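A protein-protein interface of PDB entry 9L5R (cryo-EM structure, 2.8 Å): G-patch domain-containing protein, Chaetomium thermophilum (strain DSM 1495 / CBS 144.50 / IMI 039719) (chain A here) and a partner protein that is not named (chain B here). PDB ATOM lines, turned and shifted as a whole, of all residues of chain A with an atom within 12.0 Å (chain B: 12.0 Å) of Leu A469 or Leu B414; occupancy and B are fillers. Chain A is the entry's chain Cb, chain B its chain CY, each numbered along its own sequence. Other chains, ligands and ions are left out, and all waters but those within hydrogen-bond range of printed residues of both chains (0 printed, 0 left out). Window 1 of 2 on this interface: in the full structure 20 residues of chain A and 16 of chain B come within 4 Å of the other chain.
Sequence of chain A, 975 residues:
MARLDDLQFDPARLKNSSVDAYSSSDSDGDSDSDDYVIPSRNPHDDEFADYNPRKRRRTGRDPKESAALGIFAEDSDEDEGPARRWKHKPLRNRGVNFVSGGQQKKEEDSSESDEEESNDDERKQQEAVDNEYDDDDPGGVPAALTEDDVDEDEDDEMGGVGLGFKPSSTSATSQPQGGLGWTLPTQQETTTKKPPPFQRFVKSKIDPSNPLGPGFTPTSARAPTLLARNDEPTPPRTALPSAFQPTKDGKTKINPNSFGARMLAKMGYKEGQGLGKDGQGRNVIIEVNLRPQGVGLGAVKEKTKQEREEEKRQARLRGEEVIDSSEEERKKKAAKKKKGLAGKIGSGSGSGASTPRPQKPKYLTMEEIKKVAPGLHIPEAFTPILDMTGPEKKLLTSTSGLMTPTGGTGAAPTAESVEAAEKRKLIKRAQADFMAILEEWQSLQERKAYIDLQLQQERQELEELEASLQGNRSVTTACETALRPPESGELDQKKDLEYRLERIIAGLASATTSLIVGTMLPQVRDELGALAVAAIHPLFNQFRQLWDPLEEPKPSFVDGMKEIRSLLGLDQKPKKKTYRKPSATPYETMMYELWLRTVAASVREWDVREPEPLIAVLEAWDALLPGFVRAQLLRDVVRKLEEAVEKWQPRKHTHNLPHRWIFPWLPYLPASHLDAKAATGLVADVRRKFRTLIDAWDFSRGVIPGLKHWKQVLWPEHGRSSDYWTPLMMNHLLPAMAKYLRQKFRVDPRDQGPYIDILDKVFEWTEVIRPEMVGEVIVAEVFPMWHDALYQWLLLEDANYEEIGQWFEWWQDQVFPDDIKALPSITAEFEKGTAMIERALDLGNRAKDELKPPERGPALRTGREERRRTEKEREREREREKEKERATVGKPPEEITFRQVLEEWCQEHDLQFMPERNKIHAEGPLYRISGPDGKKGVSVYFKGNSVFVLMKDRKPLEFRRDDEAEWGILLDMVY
Of the printed residues of chain B, Glu A458 touches Lys B421 (3.3 Å).
Glu A464 touches none of the printed residues of chain B.
No residue of chain B comes within 4 Å of Ala A467.
No residue of chain B comes within 4 Å of Ser A468.
Leu A469 touches just these residues of chain B: Ile B411 and Leu B414.
No residue of chain B comes within 4 Å of Gln A470.
No residue of chain B comes within 4 Å of Gly A471.
Of chain B, only Ile B411 comes within 4 Å of Asn A472.
No residue of chain A comes within 4 Å of Ala B410.
No residue of chain A comes within 4 Å of Gln B412.
No residue of chain A comes within 4 Å of Gly B413.
Leu B414 touches just these residues of chain A: Leu A465 and Leu A469.
No residue of chain A comes within 4 Å of Glu B415.
Gly B416 touches none of the printed residues of chain A.
No residue of chain A comes within 4 Å of Glu B417.
Printed residues of chain A within 4 Å of Val B418: Leu A462 (3.8 Å) and Leu A465 (3.7 Å).
Of the printed residues of chain A, Lys B421 touches Glu A458 and Leu A462.
Arg B422 touches none of the printed residues of chain A.
The nearest residue of chain B that does not touch Leu A469 is Glu B415 (4.1 Å).
Hydrophobic or aromatic side chains of chain B within 4 Å of the printed part of chain A: Ile B411, Leu B414 and Val B418.
Along chain B the printed residues that touch a printed residue of chain A span positions 411 to 421.
Printed residues of chain A that touch a printed residue of chain B: Glu A458, Leu A462, Leu A465, Leu A469 and Asn A472.
Hydrophobic or aromatic side chains of chain A that line the printed part of chain B: Leu A462, Leu A465 and Leu A469.
Among the printed residues, 8 pairs touch across the chains.
Among the printed residues, no Asp or Glu carboxylate lies within 4 Å of a Lys or Arg side-chain nitrogen of the other chain.
Among the printed residues, pairs that only touch across the chains: Glu A458 with Lys B421 (3.3 Å), Leu A465 with Leu B414 (3.5 Å), Leu A462 with Lys B421 (3.7 Å), Leu A465 with Val B418 (3.7 Å), Asn A472 with Ile B411 (3.8 Å), Leu A469 with Leu B414 (3.8 Å), Leu A462 with Val B418 (3.8 Å) and Leu A469 with Ile B411 (3.9 Å).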
ATOM      1  N   GLU A 458     -13.515 -13.607  21.301  1.00  0.00           N
ATOM      2  CA  GLU A 458     -13.866 -14.106  19.977  1.00  0.00           C
ATOM      3  C   GLU A 458     -12.693 -13.994  19.011  1.00  0.00           C
ATOM      4  O   GLU A 458     -12.498 -14.873  18.168  1.00  0.00           O
ATOM      5  CB  GLU A 458     -15.080 -13.350  19.437  1.00  0.00           C
ATOM      6  N   ARG A 459     -11.900 -12.925  19.123  1.00  0.00           N
ATOM      7  CA  ARG A 459     -10.720 -12.776  18.277  1.00  0.00           C
ATOM      8  C   ARG A 459      -9.669 -13.831  18.599  1.00  0.00           C
ATOM      9  O   ARG A 459      -9.042 -14.384  17.688  1.00  0.00           O
ATOM     10  CB  ARG A 459     -10.138 -11.372  18.434  1.00  0.00           C
ATOM     11  N   GLN A 460      -9.463 -14.122  19.888  1.00  0.00           N
ATOM     12  CA  GLN A 460      -8.526 -15.176  20.270  1.00  0.00           C
ATOM     13  C   GLN A 460      -8.993 -16.541  19.774  1.00  0.00           C
ATOM     14  O   GLN A 460      -8.189 -17.332  19.254  1.00  0.00           O
ATOM     15  CB  GLN A 460      -8.344 -15.191  21.787  1.00  0.00           C
ATOM     16  N   GLU A 461     -10.292 -16.828  19.912  1.00  0.00           N
ATOM     17  CA  GLU A 461     -10.833 -18.095  19.425  1.00  0.00           C
ATOM     18  C   GLU A 461     -10.736 -18.195  17.906  1.00  0.00           C
ATOM     19  O   GLU A 461     -10.424 -19.264  17.368  1.00  0.00           O
ATOM     20  CB  GLU A 461     -12.283 -18.254  19.881  1.00  0.00           C
ATOM     21  N   LEU A 462     -10.991 -17.087  17.202  1.00  0.00           N
ATOM     22  CA  LEU A 462     -10.876 -17.072  15.747  1.00  0.00           C
ATOM     23  C   LEU A 462      -9.438 -17.286  15.301  1.00  0.00           C
ATOM     24  O   LEU A 462      -9.191 -18.003  14.327  1.00  0.00           O
ATOM     25  CB  LEU A 462     -11.414 -15.754  15.192  1.00  0.00           C
ATOM     26  N   GLU A 463      -8.477 -16.673  16.000  1.00  0.00           N
ATOM     27  CA  GLU A 463      -7.070 -16.868  15.662  1.00  0.00           C
ATOM     28  C   GLU A 463      -6.639 -18.313  15.890  1.00  0.00           C
ATOM     29  O   GLU A 463      -5.940 -18.897  15.051  1.00  0.00           O
ATOM     30  CB  GLU A 463      -6.198 -15.913  16.477  1.00  0.00           C
ATOM     31  N   GLU A 464      -7.061 -18.908  17.011  1.00  0.00           N
ATOM     32  CA  GLU A 464      -6.717 -20.302  17.285  1.00  0.00           C
ATOM     33  C   GLU A 464      -7.346 -21.244  16.263  1.00  0.00           C
ATOM     34  O   GLU A 464      -6.685 -22.168  15.768  1.00  0.00           O
ATOM     35  CB  GLU A 464      -7.151 -20.679  18.701  1.00  0.00           C
ATOM     36  N   LEU A 465      -8.618 -21.013  15.921  1.00  0.00           N
ATOM     37  CA  LEU A 465      -9.296 -21.859  14.945  1.00  0.00           C
ATOM     38  C   LEU A 465      -8.702 -21.691  13.552  1.00  0.00           C
ATOM     39  O   LEU A 465      -8.595 -22.665  12.801  1.00  0.00           O
ATOM     40  CB  LEU A 465     -10.794 -21.550  14.934  1.00  0.00           C
ATOM     41  N   GLU A 466      -8.300 -20.468  13.192  1.00  0.00           N
ATOM     42  CA  GLU A 466      -7.670 -20.238  11.897  1.00  0.00           C
ATOM     43  C   GLU A 466      -6.303 -20.906  11.819  1.00  0.00           C
ATOM     44  O   GLU A 466      -5.944 -21.463  10.776  1.00  0.00           O
ATOM     45  CB  GLU A 466      -7.550 -18.737  11.631  1.00  0.00           C
ATOM     46  N   ALA A 467      -5.530 -20.864  12.910  1.00  0.00           N
ATOM     47  CA  ALA A 467      -4.243 -21.553  12.934  1.00  0.00           C
ATOM     48  C   ALA A 467      -4.420 -23.063  12.819  1.00  0.00           C
ATOM     49  O   ALA A 467      -3.682 -23.730  12.078  1.00  0.00           O
ATOM     50  CB  ALA A 467      -3.479 -21.197  14.208  1.00  0.00           C
ATOM     51  N   SER A 468      -5.406 -23.616  13.535  1.00  0.00           N
ATOM     52  CA  SER A 468      -5.677 -25.050  13.447  1.00  0.00           C
ATOM     53  C   SER A 468      -6.148 -25.444  12.050  1.00  0.00           C
ATOM     54  O   SER A 468      -5.745 -26.488  11.524  1.00  0.00           O
ATOM     55  CB  SER A 468      -6.713 -25.451  14.497  1.00  0.00           C
ATOM     56  N   LEU A 469      -6.998 -24.616  11.433  1.00  0.00           N
ATOM     57  CA  LEU A 469      -7.481 -24.900  10.086  1.00  0.00           C
ATOM     58  C   LEU A 469      -6.357 -24.808   9.060  1.00  0.00           C
ATOM     59  O   LEU A 469      -6.310 -25.608   8.119  1.00  0.00           O
ATOM     60  CB  LEU A 469      -8.617 -23.944   9.725  1.00  0.00           C
ATOM     61  N   GLN A 470      -5.448 -23.842   9.222  1.00  0.00           N
ATOM     62  CA  GLN A 470      -4.300 -23.741   8.327  1.00  0.00           C
ATOM     63  C   GLN A 470      -3.376 -24.946   8.468  1.00  0.00           C
ATOM     64  O   GLN A 470      -2.882 -25.476   7.465  1.00  0.00           O
ATOM     65  CB  GLN A 470      -3.536 -22.445   8.598  1.00  0.00           C
ATOM     66  N   GLY A 471      -3.141 -25.397   9.706  1.00  0.00           N
ATOM     67  CA  GLY A 471      -2.338 -26.595   9.906  1.00  0.00           C
ATOM     68  C   GLY A 471      -2.979 -27.839   9.319  1.00  0.00           C
ATOM     69  O   GLY A 471      -2.302 -28.669   8.704  1.00  0.00           O
ATOM     70  N   ASN A 472      -4.299 -27.978   9.487  1.00  0.00           N
ATOM     71  CA  ASN A 472      -5.008 -29.120   8.918  1.00  0.00           C
ATOM     72  C   ASN A 472      -5.014 -29.071   7.394  1.00  0.00           C
ATOM     73  O   ASN A 472      -4.910 -30.111   6.735  1.00  0.00           O
ATOM     74  CB  ASN A 472      -6.435 -29.175   9.462  1.00  0.00           C
ATOM     75  N   ARG A 473      -5.136 -27.871   6.817  1.00  0.00           N
ATOM     76  CA  ARG A 473      -5.070 -27.727   5.366  1.00  0.00           C
ATOM     77  C   ARG A 473      -3.686 -28.080   4.837  1.00  0.00           C
ATOM     78  O   ARG A 473      -3.564 -28.716   3.784  1.00  0.00           O
ATOM     79  CB  ARG A 473      -5.451 -26.303   4.963  1.00  0.00           C
ATOM     80  N   SER A 474      -2.632 -27.673   5.552  1.00  0.00           N
ATOM     81  CA  SER A 474      -1.276 -28.041   5.152  1.00  0.00           C
ATOM     82  C   SER A 474      -1.059 -29.548   5.248  1.00  0.00           C
ATOM     83  O   SER A 474      -0.416 -30.146   4.375  1.00  0.00           O
ATOM     84  CB  SER A 474      -0.256 -27.296   6.013  1.00  0.00           C
ATOM     85  N   VAL A 475      -1.598 -30.176   6.296  1.00  0.00           N
ATOM     86  CA  VAL A 475      -1.484 -31.626   6.445  1.00  0.00           C
ATOM     87  C   VAL A 475      -2.241 -32.345   5.334  1.00  0.00           C
ATOM     88  O   VAL A 475      -1.767 -33.351   4.794  1.00  0.00           O
ATOM     89  CB  VAL A 475      -1.975 -32.058   7.838  1.00  0.00           C
ATOM     90  N   THR A 476      -3.428 -31.844   4.977  1.00  0.00           N
ATOM     91  CA  THR A 476      -4.199 -32.435   3.888  1.00  0.00           C
ATOM     92  C   THR A 476      -3.492 -32.267   2.547  1.00  0.00           C
ATOM     93  O   THR A 476      -3.516 -33.177   1.710  1.00  0.00           O
ATOM     94  CB  THR A 476      -5.596 -31.816   3.835  1.00  0.00           C
ATOM     95  N   THR A 477      -2.863 -31.109   2.323  1.00  0.00           N
ATOM     96  CA  THR A 477      -2.103 -30.895   1.095  1.00  0.00           C
ATOM     97  C   THR A 477      -0.897 -31.826   1.020  1.00  0.00           C
ATOM     98  O   THR A 477      -0.594 -32.371  -0.050  1.00  0.00           O
ATOM     99  CB  THR A 477      -1.656 -29.437   0.999  1.00  0.00           C
ATOM    100  N   ALA A 478      -0.203 -32.023   2.145  1.00  0.00           N
ATOM    101  CA  ALA A 478       0.916 -32.961   2.176  1.00  0.00           C
ATOM    102  C   ALA A 478       0.447 -34.393   1.937  1.00  0.00           C
ATOM    103  O   ALA A 478       1.120 -35.163   1.240  1.00  0.00           O
ATOM    104  CB  ALA A 478       1.654 -32.853   3.510  1.00  0.00           C
ATOM    105  N   THR A 519       4.465 -30.632  18.510  1.00  0.00           N
ATOM    106  CA  THR A 519       3.413 -29.864  17.858  1.00  0.00           C
ATOM    107  C   THR A 519       2.397 -30.739  17.138  1.00  0.00           C
ATOM    108  O   THR A 519       1.480 -30.207  16.504  1.00  0.00           O
ATOM    109  CB  THR A 519       4.021 -28.866  16.866  1.00  0.00           C
ATOM    110  N   LEU A 521      -0.674 -33.357  17.277  1.00  0.00           N
ATOM    111  CA  LEU A 521      -1.715 -33.845  18.164  1.00  0.00           C
ATOM    112  C   LEU A 521      -1.755 -35.373  18.146  1.00  0.00           C
ATOM    113  O   LEU A 521      -1.420 -35.998  17.135  1.00  0.00           O
ATOM    114  CB  LEU A 521      -3.073 -33.283  17.754  1.00  0.00           C
ATOM    115  N   VAL A 524      -4.166 -36.600  15.437  1.00  0.00           N
ATOM    116  CA  VAL A 524      -3.576 -36.496  14.106  1.00  0.00           C
ATOM    117  C   VAL A 524      -2.516 -37.572  13.904  1.00  0.00           C
ATOM    118  O   VAL A 524      -2.382 -38.128  12.807  1.00  0.00           O
ATOM    119  CB  VAL A 524      -2.998 -35.086  13.887  1.00  0.00           C
ATOM    120  N   LEU B 404      -8.902 -39.027   4.762  1.00  0.00           N
ATOM    121  CA  LEU B 404      -8.747 -37.713   4.143  1.00  0.00           C
ATOM    122  C   LEU B 404     -10.024 -36.888   4.267  1.00  0.00           C
ATOM    123  O   LEU B 404      -9.967 -35.676   4.508  1.00  0.00           O
ATOM    124  CB  LEU B 404      -8.347 -37.869   2.676  1.00  0.00           C
ATOM    125  N   GLN B 405     -11.184 -37.530   4.110  1.00  0.00           N
ATOM    126  CA  GLN B 405     -12.455 -36.831   4.279  1.00  0.00           C
ATOM    127  C   GLN B 405     -12.655 -36.375   5.721  1.00  0.00           C
ATOM    128  O   GLN B 405     -13.180 -35.285   5.959  1.00  0.00           O
ATOM    129  CB  GLN B 405     -13.612 -37.727   3.833  1.00  0.00           C
ATOM    130  N   ARG B 406     -12.246 -37.197   6.693  1.00  0.00           N
ATOM    131  CA  ARG B 406     -12.342 -36.805   8.097  1.00  0.00           C
ATOM    132  C   ARG B 406     -11.429 -35.624   8.408  1.00  0.00           C
ATOM    133  O   ARG B 406     -11.817 -34.710   9.148  1.00  0.00           O
ATOM    134  CB  ARG B 406     -12.006 -37.994   8.996  1.00  0.00           C
ATOM    135  N   ILE B 407     -10.217 -35.624   7.844  1.00  0.00           N
ATOM    136  CA  ILE B 407      -9.300 -34.499   8.034  1.00  0.00           C
ATOM    137  C   ILE B 407      -9.867 -33.229   7.406  1.00  0.00           C
ATOM    138  O   ILE B 407      -9.815 -32.145   8.005  1.00  0.00           O
ATOM    139  CB  ILE B 407      -7.912 -34.841   7.465  1.00  0.00           C
ATOM    140  N   ARG B 408     -10.425 -33.345   6.196  1.00  0.00           N
ATOM    141  CA  ARG B 408     -11.011 -32.184   5.529  1.00  0.00           C
ATOM    142  C   ARG B 408     -12.242 -31.678   6.271  1.00  0.00           C
ATOM    143  O   ARG B 408     -12.482 -30.467   6.330  1.00  0.00           O
ATOM    144  CB  ARG B 408     -11.363 -32.533   4.083  1.00  0.00           C
ATOM    145  N   GLU B 409     -13.028 -32.588   6.851  1.00  0.00           N
ATOM    146  CA  GLU B 409     -14.190 -32.187   7.635  1.00  0.00           C
ATOM    147  C   GLU B 409     -13.775 -31.475   8.916  1.00  0.00           C
ATOM    148  O   GLU B 409     -14.419 -30.503   9.324  1.00  0.00           O
ATOM    149  CB  GLU B 409     -15.055 -33.406   7.952  1.00  0.00           C
ATOM    150  N   ALA B 410     -12.702 -31.944   9.562  1.00  0.00           N
ATOM    151  CA  ALA B 410     -12.184 -31.244  10.736  1.00  0.00           C
ATOM    152  C   ALA B 410     -11.667 -29.857  10.370  1.00  0.00           C
ATOM    153  O   ALA B 410     -11.874 -28.890  11.116  1.00  0.00           O
ATOM    154  CB  ALA B 410     -11.084 -32.073  11.400  1.00  0.00           C
ATOM    155  N   ILE B 411     -11.004 -29.740   9.214  1.00  0.00           N
ATOM    156  CA  ILE B 411     -10.516 -28.441   8.751  1.00  0.00           C
ATOM    157  C   ILE B 411     -11.680 -27.499   8.460  1.00  0.00           C
ATOM    158  O   ILE B 411     -11.640 -26.312   8.808  1.00  0.00           O
ATOM    159  CB  ILE B 411      -9.613 -28.620   7.518  1.00  0.00           C
ATOM    160  N   GLN B 412     -12.734 -28.013   7.820  1.00  0.00           N
ATOM    161  CA  GLN B 412     -13.903 -27.190   7.522  1.00  0.00           C
ATOM    162  C   GLN B 412     -14.644 -26.790   8.793  1.00  0.00           C
ATOM    163  O   GLN B 412     -15.178 -25.679   8.879  1.00  0.00           O
ATOM    164  CB  GLN B 412     -14.836 -27.933   6.564  1.00  0.00           C
ATOM    165  N   GLY B 413     -14.688 -27.679   9.787  1.00  0.00           N
ATOM    166  CA  GLY B 413     -15.286 -27.319  11.064  1.00  0.00           C
ATOM    167  C   GLY B 413     -14.503 -26.244  11.793  1.00  0.00           C
ATOM    168  O   GLY B 413     -15.088 -25.336  12.391  1.00  0.00           O
ATOM    169  N   LEU B 414     -13.169 -26.331  11.751  1.00  0.00           N
ATOM    170  CA  LEU B 414     -12.339 -25.275  12.325  1.00  0.00           C
ATOM    171  C   LEU B 414     -12.540 -23.953  11.591  1.00  0.00           C
ATOM    172  O   LEU B 414     -12.588 -22.888  12.219  1.00  0.00           O
ATOM    173  CB  LEU B 414     -10.869 -25.690  12.294  1.00  0.00           C
ATOM    174  N   GLU B 415     -12.670 -24.005  10.261  1.00  0.00           N
ATOM    175  CA  GLU B 415     -12.929 -22.796   9.482  1.00  0.00           C
ATOM    176  C   GLU B 415     -14.287 -22.191   9.823  1.00  0.00           C
ATOM    177  O   GLU B 415     -14.419 -20.966   9.923  1.00  0.00           O
ATOM    178  CB  GLU B 415     -12.842 -23.107   7.989  1.00  0.00           C
ATOM    179  N   GLY B 416     -15.304 -23.035  10.006  1.00  0.00           N
ATOM    180  CA  GLY B 416     -16.612 -22.535  10.396  1.00  0.00           C
ATOM    181  C   GLY B 416     -16.618 -21.933  11.788  1.00  0.00           C
ATOM    182  O   GLY B 416     -17.282 -20.923  12.033  1.00  0.00           O
ATOM    183  N   GLU B 417     -15.875 -22.544  12.717  1.00  0.00           N
ATOM    184  CA  GLU B 417     -15.737 -21.972  14.054  1.00  0.00           C
ATOM    185  C   GLU B 417     -15.015 -20.630  14.009  1.00  0.00           C
ATOM    186  O   GLU B 417     -15.381 -19.696  14.732  1.00  0.00           O
ATOM    187  CB  GLU B 417     -14.998 -22.949  14.968  1.00  0.00           C
ATOM    188  N   VAL B 418     -13.992 -20.517  13.155  1.00  0.00           N
ATOM    189  CA  VAL B 418     -13.279 -19.251  12.993  1.00  0.00           C
ATOM    190  C   VAL B 418     -14.198 -18.186  12.407  1.00  0.00           C
ATOM    191  O   VAL B 418     -14.164 -17.022  12.821  1.00  0.00           O
ATOM    192  CB  VAL B 418     -12.025 -19.451  12.123  1.00  0.00           C
ATOM    193  N   VAL B 419     -15.030 -18.569  11.434  1.00  0.00           N
ATOM    194  CA  VAL B 419     -15.970 -17.628  10.830  1.00  0.00           C
ATOM    195  C   VAL B 419     -17.012 -17.175  11.847  1.00  0.00           C
ATOM    196  O   VAL B 419     -17.378 -15.993  11.894  1.00  0.00           O
ATOM    197  CB  VAL B 419     -16.628 -18.257   9.588  1.00  0.00           C
ATOM    198  N   ARG B 420     -17.508 -18.104  12.670  1.00  0.00           N
ATOM    199  CA  ARG B 420     -18.475 -17.750  13.706  1.00  0.00           C
ATOM    200  C   ARG B 420     -17.858 -16.827  14.751  1.00  0.00           C
ATOM    201  O   ARG B 420     -18.502 -15.873  15.203  1.00  0.00           O
ATOM    202  CB  ARG B 420     -19.022 -19.016  14.365  1.00  0.00           C
ATOM    203  N   LYS B 421     -16.607 -17.092  15.139  1.00  0.00           N
ATOM    204  CA  LYS B 421     -15.929 -16.223  16.095  1.00  0.00           C
ATOM    205  C   LYS B 421     -15.662 -14.843  15.502  1.00  0.00           C
ATOM    206  O   LYS B 421     -15.762 -13.833  16.207  1.00  0.00           O
ATOM    207  CB  LYS B 421     -14.627 -16.874  16.559  1.00  0.00           C
ATOM    208  N   ARG B 422     -15.327 -14.780  14.210  1.00  0.00           N
ATOM    209  CA  ARG B 422     -15.135 -13.493  13.548  1.00  0.00           C
ATOM    210  C   ARG B 422     -16.439 -12.706  13.469  1.00  0.00           C
ATOM    211  O   ARG B 422     -16.446 -11.486  13.670  1.00  0.00           O
ATOM    212  CB  ARG B 422     -14.551 -13.704  12.152  1.00  0.00           C
ATOM    213  N   SER B 423     -17.551 -13.389  13.177  1.00  0.00           N
ATOM    214  CA  SER B 423     -18.852 -12.726  13.159  1.00  0.00           C
ATOM    215  C   SER B 423     -19.242 -12.232  14.548  1.00  0.00           C
ATOM    216  O   SER B 423     -19.798 -11.136  14.690  1.00  0.00           O
ATOM    217  CB  SER B 423     -19.916 -13.673  12.607  1.00  0.00           C
